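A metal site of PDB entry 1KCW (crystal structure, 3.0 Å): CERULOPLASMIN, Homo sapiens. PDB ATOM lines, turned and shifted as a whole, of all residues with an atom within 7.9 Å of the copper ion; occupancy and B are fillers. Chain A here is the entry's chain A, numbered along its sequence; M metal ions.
N of Gly 638 sits close to SG of Cys 680, at 3.6 Å.
The backbone carbonyl oxygen of Ala 634 sits at hydrogen-bond distance from a ring nitrogen (NE2) of His 685 (3.0 Å).
A ring nitrogen (NE2) of His 685 sits at hydrogen-bond distance from the side-chain carboxylate (OE2) of Glu 971.
SD of Met 690 lies close to ND1 of His 637, at 3.8 Å.
A ring nitrogen (NE2) of His 637 sits at hydrogen-bond distance from the backbone carbonyl oxygen (O) of Pro 563, 3.5 Å away.
NE2 of His 637 is in hydrogen-bond range of OD1 of Asp 635 (3.2 Å).
The backbone NH (N) of His 637 lies within hydrogen-bond range of the backbone carbonyl oxygen (O) of Leu 658 (2.8 Å).
NE2 of His 637 lies within hydrogen-bond range of OG of Ser 629, at 3.4 Å.
Met 690 touches the copper ion.
The copper ion is bound by the side-chain sulfur of Cys 680 (2.0 Å), a ring nitrogen (ND1) of His 685 (2.1 Å) and a ring nitrogen (ND1) of His 637 (2.1 Å).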
ATOM      1  N   PRO A 563      36.503 -10.678  10.854  1.00  0.00           N
ATOM      2  CA  PRO A 563      35.536 -10.959   9.794  1.00  0.00           C
ATOM      3  C   PRO A 563      35.212  -9.622   9.133  1.00  0.00           C
ATOM      4  O   PRO A 563      34.953  -8.649   9.839  1.00  0.00           O
ATOM      5  CB  PRO A 563      34.342 -11.517  10.558  1.00  0.00           C
ATOM      6  CG  PRO A 563      34.425 -10.813  11.865  1.00  0.00           C
ATOM      7  CD  PRO A 563      35.886 -10.722  12.188  1.00  0.00           C
ATOM      8  N   THR A 564      35.266  -9.558   7.803  1.00  0.00           N
ATOM      9  CA  THR A 564      35.018  -8.325   7.065  1.00  0.00           C
ATOM     10  C   THR A 564      34.700  -8.661   5.636  1.00  0.00           C
ATOM     11  O   THR A 564      34.735  -9.832   5.253  1.00  0.00           O
ATOM     12  CB  THR A 564      36.289  -7.460   6.957  1.00  0.00           C
ATOM     13  OG1 THR A 564      36.867  -7.298   8.247  1.00  0.00           O
ATOM     14  CG2 THR A 564      35.974  -6.099   6.393  1.00  0.00           C
ATOM     15  N   VAL A 565      34.323  -7.650   4.855  1.00  0.00           N
ATOM     16  CA  VAL A 565      34.081  -7.852   3.438  1.00  0.00           C
ATOM     17  C   VAL A 565      35.228  -7.129   2.791  1.00  0.00           C
ATOM     18  O   VAL A 565      35.193  -5.905   2.667  1.00  0.00           O
ATOM     19  CB  VAL A 565      32.777  -7.207   2.975  1.00  0.00           C
ATOM     20  CG1 VAL A 565      32.503  -7.576   1.513  1.00  0.00           C
ATOM     21  CG2 VAL A 565      31.632  -7.610   3.925  1.00  0.00           C
ATOM     22  N   HIS A 602      33.976 -11.494   1.022  1.00  0.00           N
ATOM     23  CA  HIS A 602      33.355 -11.781   2.318  1.00  0.00           C
ATOM     24  C   HIS A 602      34.226 -12.820   2.939  1.00  0.00           C
ATOM     25  O   HIS A 602      34.131 -13.992   2.600  1.00  0.00           O
ATOM     26  CB  HIS A 602      31.950 -12.312   2.130  1.00  0.00           C
ATOM     27  CG  HIS A 602      30.971 -11.283   1.656  1.00  0.00           C
ATOM     28  ND1 HIS A 602      30.395 -11.279   0.408  1.00  0.00           N
ATOM     29  CD2 HIS A 602      30.476 -10.194   2.293  1.00  0.00           C
ATOM     30  CE1 HIS A 602      29.572 -10.211   0.332  1.00  0.00           C
ATOM     31  NE2 HIS A 602      29.592  -9.531   1.458  1.00  0.00           N
ATOM     32  N   SER A 603      35.022 -12.426   3.920  1.00  0.00           N
ATOM     33  CA  SER A 603      35.949 -13.373   4.479  1.00  0.00           C
ATOM     34  C   SER A 603      36.285 -13.191   5.943  1.00  0.00           C
ATOM     35  O   SER A 603      36.059 -12.135   6.538  1.00  0.00           O
ATOM     36  CB  SER A 603      37.253 -13.255   3.697  1.00  0.00           C
ATOM     37  OG  SER A 603      37.856 -11.975   3.914  1.00  0.00           O
ATOM     38  N   MET A 604      36.949 -14.190   6.503  1.00  0.00           N
ATOM     39  CA  MET A 604      37.372 -14.142   7.884  1.00  0.00           C
ATOM     40  C   MET A 604      38.878 -14.338   7.902  1.00  0.00           C
ATOM     41  O   MET A 604      39.406 -15.291   7.313  1.00  0.00           O
ATOM     42  CB  MET A 604      36.675 -15.233   8.655  1.00  0.00           C
ATOM     43  CG  MET A 604      36.106 -14.728   9.944  1.00  0.00           C
ATOM     44  SD  MET A 604      35.117 -15.982  10.648  1.00  0.00           S
ATOM     45  CE  MET A 604      33.881 -16.163   9.306  1.00  0.00           C
ATOM     46  N   SER A 629      36.589  -5.852  13.956  1.00  0.00           N
ATOM     47  CA  SER A 629      36.219  -5.648  12.562  1.00  0.00           C
ATOM     48  C   SER A 629      36.359  -4.191  12.122  1.00  0.00           C
ATOM     49  O   SER A 629      36.649  -3.299  12.934  1.00  0.00           O
ATOM     50  CB  SER A 629      34.798  -6.146  12.310  1.00  0.00           C
ATOM     51  OG  SER A 629      34.345  -5.821  11.004  1.00  0.00           O
ATOM     52  N   ALA A 634      28.027  -2.229   5.797  1.00  0.00           N
ATOM     53  CA  ALA A 634      27.636  -3.597   5.474  1.00  0.00           C
ATOM     54  C   ALA A 634      28.289  -4.544   6.456  1.00  0.00           C
ATOM     55  O   ALA A 634      28.120  -5.764   6.361  1.00  0.00           O
ATOM     56  CB  ALA A 634      28.026  -3.973   4.073  1.00  0.00           C
ATOM     57  N   ASP A 635      29.079  -3.970   7.359  1.00  0.00           N
ATOM     58  CA  ASP A 635      29.764  -4.752   8.342  1.00  0.00           C
ATOM     59  C   ASP A 635      28.956  -4.860   9.620  1.00  0.00           C
ATOM     60  O   ASP A 635      29.276  -4.225  10.654  1.00  0.00           O
ATOM     61  CB  ASP A 635      31.192  -4.251   8.558  1.00  0.00           C
ATOM     62  CG  ASP A 635      32.089  -4.596   7.379  1.00  0.00           C
ATOM     63  OD1 ASP A 635      32.367  -5.788   7.162  1.00  0.00           O
ATOM     64  OD2 ASP A 635      32.488  -3.699   6.612  1.00  0.00           O
ATOM     65  N   VAL A 636      27.831  -5.579   9.506  1.00  0.00           N
ATOM     66  CA  VAL A 636      26.966  -5.882  10.646  1.00  0.00           C
ATOM     67  C   VAL A 636      27.055  -7.422  10.741  1.00  0.00           C
ATOM     68  O   VAL A 636      26.421  -8.150   9.957  1.00  0.00           O
ATOM     69  CB  VAL A 636      25.444  -5.351  10.494  1.00  0.00           C
ATOM     70  CG1 VAL A 636      25.432  -3.861  10.199  1.00  0.00           C
ATOM     71  CG2 VAL A 636      24.661  -6.073   9.425  1.00  0.00           C
ATOM     72  N   HIS A 637      27.915  -7.915  11.609  1.00  0.00           N
ATOM     73  CA  HIS A 637      28.026  -9.358  11.699  1.00  0.00           C
ATOM     74  C   HIS A 637      27.571  -9.960  12.998  1.00  0.00           C
ATOM     75  O   HIS A 637      27.635  -9.353  14.071  1.00  0.00           O
ATOM     76  CB  HIS A 637      29.464  -9.869  11.455  1.00  0.00           C
ATOM     77  CG  HIS A 637      30.284  -8.997  10.564  1.00  0.00           C
ATOM     78  ND1 HIS A 637      30.338  -9.207   9.212  1.00  0.00           N
ATOM     79  CD2 HIS A 637      31.092  -7.969  10.902  1.00  0.00           C
ATOM     80  CE1 HIS A 637      31.180  -8.314   8.760  1.00  0.00           C
ATOM     81  NE2 HIS A 637      31.667  -7.536   9.748  1.00  0.00           N
ATOM     82  N   GLY A 638      27.232 -11.245  12.873  1.00  0.00           N
ATOM     83  CA  GLY A 638      26.830 -12.049  13.999  1.00  0.00           C
ATOM     84  C   GLY A 638      27.675 -13.309  13.953  1.00  0.00           C
ATOM     85  O   GLY A 638      27.346 -14.269  13.233  1.00  0.00           O
ATOM     86  N   ILE A 639      28.808 -13.285  14.641  1.00  0.00           N
ATOM     87  CA  ILE A 639      29.714 -14.434  14.678  1.00  0.00           C
ATOM     88  C   ILE A 639      29.161 -15.491  15.638  1.00  0.00           C
ATOM     89  O   ILE A 639      29.067 -15.287  16.823  1.00  0.00           O
ATOM     90  CB  ILE A 639      31.137 -14.002  15.059  1.00  0.00           C
ATOM     91  CG1 ILE A 639      31.643 -12.940  14.065  1.00  0.00           C
ATOM     92  CG2 ILE A 639      32.055 -15.182  15.048  1.00  0.00           C
ATOM     93  CD1 ILE A 639      31.527 -13.333  12.594  1.00  0.00           C
ATOM     94  N   LEU A 658      29.473  -7.658  15.632  1.00  0.00           N
ATOM     95  CA  LEU A 658      30.554  -6.775  15.254  1.00  0.00           C
ATOM     96  C   LEU A 658      30.169  -5.854  14.109  1.00  0.00           C
ATOM     97  O   LEU A 658      29.530  -6.262  13.129  1.00  0.00           O
ATOM     98  CB  LEU A 658      31.781  -7.597  14.876  1.00  0.00           C
ATOM     99  CG  LEU A 658      32.438  -8.257  16.089  1.00  0.00           C
ATOM    100  CD1 LEU A 658      33.583  -9.129  15.696  1.00  0.00           C
ATOM    101  CD2 LEU A 658      32.919  -7.183  17.001  1.00  0.00           C
ATOM    102  N   GLU A 679      30.724 -19.096  12.447  1.00  0.00           N
ATOM    103  CA  GLU A 679      30.212 -18.477  11.233  1.00  0.00           C
ATOM    104  C   GLU A 679      29.586 -17.127  11.486  1.00  0.00           C
ATOM    105  O   GLU A 679      29.429 -16.727  12.634  1.00  0.00           O
ATOM    106  CB  GLU A 679      29.175 -19.393  10.616  1.00  0.00           C
ATOM    107  CG  GLU A 679      28.299 -20.051  11.632  1.00  0.00           C
ATOM    108  CD  GLU A 679      27.166 -20.857  11.001  1.00  0.00           C
ATOM    109  OE1 GLU A 679      27.419 -21.919  10.372  1.00  0.00           O
ATOM    110  OE2 GLU A 679      26.004 -20.416  11.160  1.00  0.00           O
ATOM    111  N   CYS A 680      29.336 -16.383  10.418  1.00  0.00           N
ATOM    112  CA  CYS A 680      28.661 -15.107  10.553  1.00  0.00           C
ATOM    113  C   CYS A 680      27.225 -15.421  10.124  1.00  0.00           C
ATOM    114  O   CYS A 680      26.988 -15.894   8.989  1.00  0.00           O
ATOM    115  CB  CYS A 680      29.267 -14.021   9.675  1.00  0.00           C
ATOM    116  SG  CYS A 680      28.320 -12.489   9.687  1.00  0.00           S
ATOM    117  N   LEU A 681      26.311 -15.321  11.086  1.00  0.00           N
ATOM    118  CA  LEU A 681      24.892 -15.584  10.893  1.00  0.00           C
ATOM    119  C   LEU A 681      24.193 -14.742   9.855  1.00  0.00           C
ATOM    120  O   LEU A 681      23.251 -15.240   9.204  1.00  0.00           O
ATOM    121  CB  LEU A 681      24.150 -15.364  12.188  1.00  0.00           C
ATOM    122  CG  LEU A 681      24.005 -16.568  13.082  1.00  0.00           C
ATOM    123  CD1 LEU A 681      23.230 -16.134  14.289  1.00  0.00           C
ATOM    124  CD2 LEU A 681      23.311 -17.708  12.342  1.00  0.00           C
ATOM    125  N   THR A 682      24.610 -13.481   9.747  1.00  0.00           N
ATOM    126  CA  THR A 682      23.975 -12.539   8.842  1.00  0.00           C
ATOM    127  C   THR A 682      24.126 -13.020   7.409  1.00  0.00           C
ATOM    128  O   THR A 682      25.216 -12.983   6.840  1.00  0.00           O
ATOM    129  CB  THR A 682      24.478 -11.086   9.070  1.00  0.00           C
ATOM    130  OG1 THR A 682      25.227 -10.652   7.923  1.00  0.00           O
ATOM    131  CG2 THR A 682      25.346 -11.007  10.315  1.00  0.00           C
ATOM    132  N   THR A 683      22.996 -13.452   6.913  1.00  0.00           N
ATOM    133  CA  THR A 683      22.793 -14.012   5.595  1.00  0.00           C
ATOM    134  C   THR A 683      23.882 -13.745   4.514  1.00  0.00           C
ATOM    135  O   THR A 683      24.775 -14.566   4.300  1.00  0.00           O
ATOM    136  CB  THR A 683      21.448 -13.545   5.043  1.00  0.00           C
ATOM    137  OG1 THR A 683      20.413 -13.916   5.979  1.00  0.00           O
ATOM    138  CG2 THR A 683      21.175 -14.167   3.692  1.00  0.00           C
ATOM    139  N   ASP A 684      23.785 -12.618   3.767  1.00  0.00           N
ATOM    140  CA  ASP A 684      24.743 -12.276   2.667  1.00  0.00           C
ATOM    141  C   ASP A 684      26.138 -12.817   2.955  1.00  0.00           C
ATOM    142  O   ASP A 684      26.700 -13.527   2.124  1.00  0.00           O
ATOM    143  CB  ASP A 684      24.743 -10.737   2.448  1.00  0.00           C
ATOM    144  CG  ASP A 684      25.896 -10.191   1.581  1.00  0.00           C
ATOM    145  OD1 ASP A 684      25.772 -10.189   0.330  1.00  0.00           O
ATOM    146  OD2 ASP A 684      26.922  -9.727   2.149  1.00  0.00           O
ATOM    147  N   HIS A 685      26.410 -12.452   4.229  1.00  0.00           N
ATOM    148  CA  HIS A 685      27.778 -12.818   4.624  1.00  0.00           C
ATOM    149  C   HIS A 685      27.964 -14.336   4.633  1.00  0.00           C
ATOM    150  O   HIS A 685      28.930 -14.846   4.086  1.00  0.00           O
ATOM    151  CB  HIS A 685      28.116 -12.258   6.013  1.00  0.00           C
ATOM    152  CG  HIS A 685      27.984 -10.770   6.092  1.00  0.00           C
ATOM    153  ND1 HIS A 685      28.582 -10.059   7.097  1.00  0.00           N
ATOM    154  CD2 HIS A 685      27.367  -9.912   5.238  1.00  0.00           C
ATOM    155  CE1 HIS A 685      28.339  -8.787   6.833  1.00  0.00           C
ATOM    156  NE2 HIS A 685      27.606  -8.648   5.717  1.00  0.00           N
ATOM    157  N   TYR A 686      27.012 -15.063   5.182  1.00  0.00           N
ATOM    158  CA  TYR A 686      27.144 -16.510   5.210  1.00  0.00           C
ATOM    159  C   TYR A 686      27.148 -17.094   3.810  1.00  0.00           C
ATOM    160  O   TYR A 686      27.940 -17.958   3.492  1.00  0.00           O
ATOM    161  CB  TYR A 686      26.012 -17.135   6.020  1.00  0.00           C
ATOM    162  CG  TYR A 686      26.088 -18.623   6.139  1.00  0.00           C
ATOM    163  CD1 TYR A 686      26.908 -19.211   7.088  1.00  0.00           C
ATOM    164  CD2 TYR A 686      25.312 -19.440   5.360  1.00  0.00           C
ATOM    165  CE1 TYR A 686      26.926 -20.584   7.260  1.00  0.00           C
ATOM    166  CE2 TYR A 686      25.321 -20.804   5.520  1.00  0.00           C
ATOM    167  CZ  TYR A 686      26.123 -21.366   6.469  1.00  0.00           C
ATOM    168  OH  TYR A 686      26.092 -22.729   6.679  1.00  0.00           O
ATOM    169  N   MET A 690      31.365 -16.398   4.515  1.00  0.00           N
ATOM    170  CA  MET A 690      31.921 -16.020   5.794  1.00  0.00           C
ATOM    171  C   MET A 690      31.771 -17.095   6.879  1.00  0.00           C
ATOM    172  O   MET A 690      31.338 -16.795   7.996  1.00  0.00           O
ATOM    173  CB  MET A 690      31.365 -14.681   6.272  1.00  0.00           C
ATOM    174  CG  MET A 690      32.201 -14.048   7.378  1.00  0.00           C
ATOM    175  SD  MET A 690      31.810 -12.333   7.711  1.00  0.00           S
ATOM    176  CE  MET A 690      31.913 -11.688   6.093  1.00  0.00           C
ATOM    177  N   GLU A 971      21.957  -8.107   6.513  1.00  0.00           N
ATOM    178  CA  GLU A 971      22.667  -6.874   6.959  1.00  0.00           C
ATOM    179  C   GLU A 971      21.814  -5.731   7.411  1.00  0.00           C
ATOM    180  O   GLU A 971      22.242  -4.875   8.181  1.00  0.00           O
ATOM    181  CB  GLU A 971      23.533  -6.316   5.853  1.00  0.00           C
ATOM    182  CG  GLU A 971      24.567  -7.240   5.399  1.00  0.00           C
ATOM    183  CD  GLU A 971      25.181  -6.790   4.126  1.00  0.00           C
ATOM    184  OE1 GLU A 971      24.428  -6.667   3.141  1.00  0.00           O
ATOM    185  OE2 GLU A 971      26.420  -6.565   4.121  1.00  0.00           O
HETATM  186 CU    CU M   1      29.298 -10.955   8.804  1.00  0.00          CU
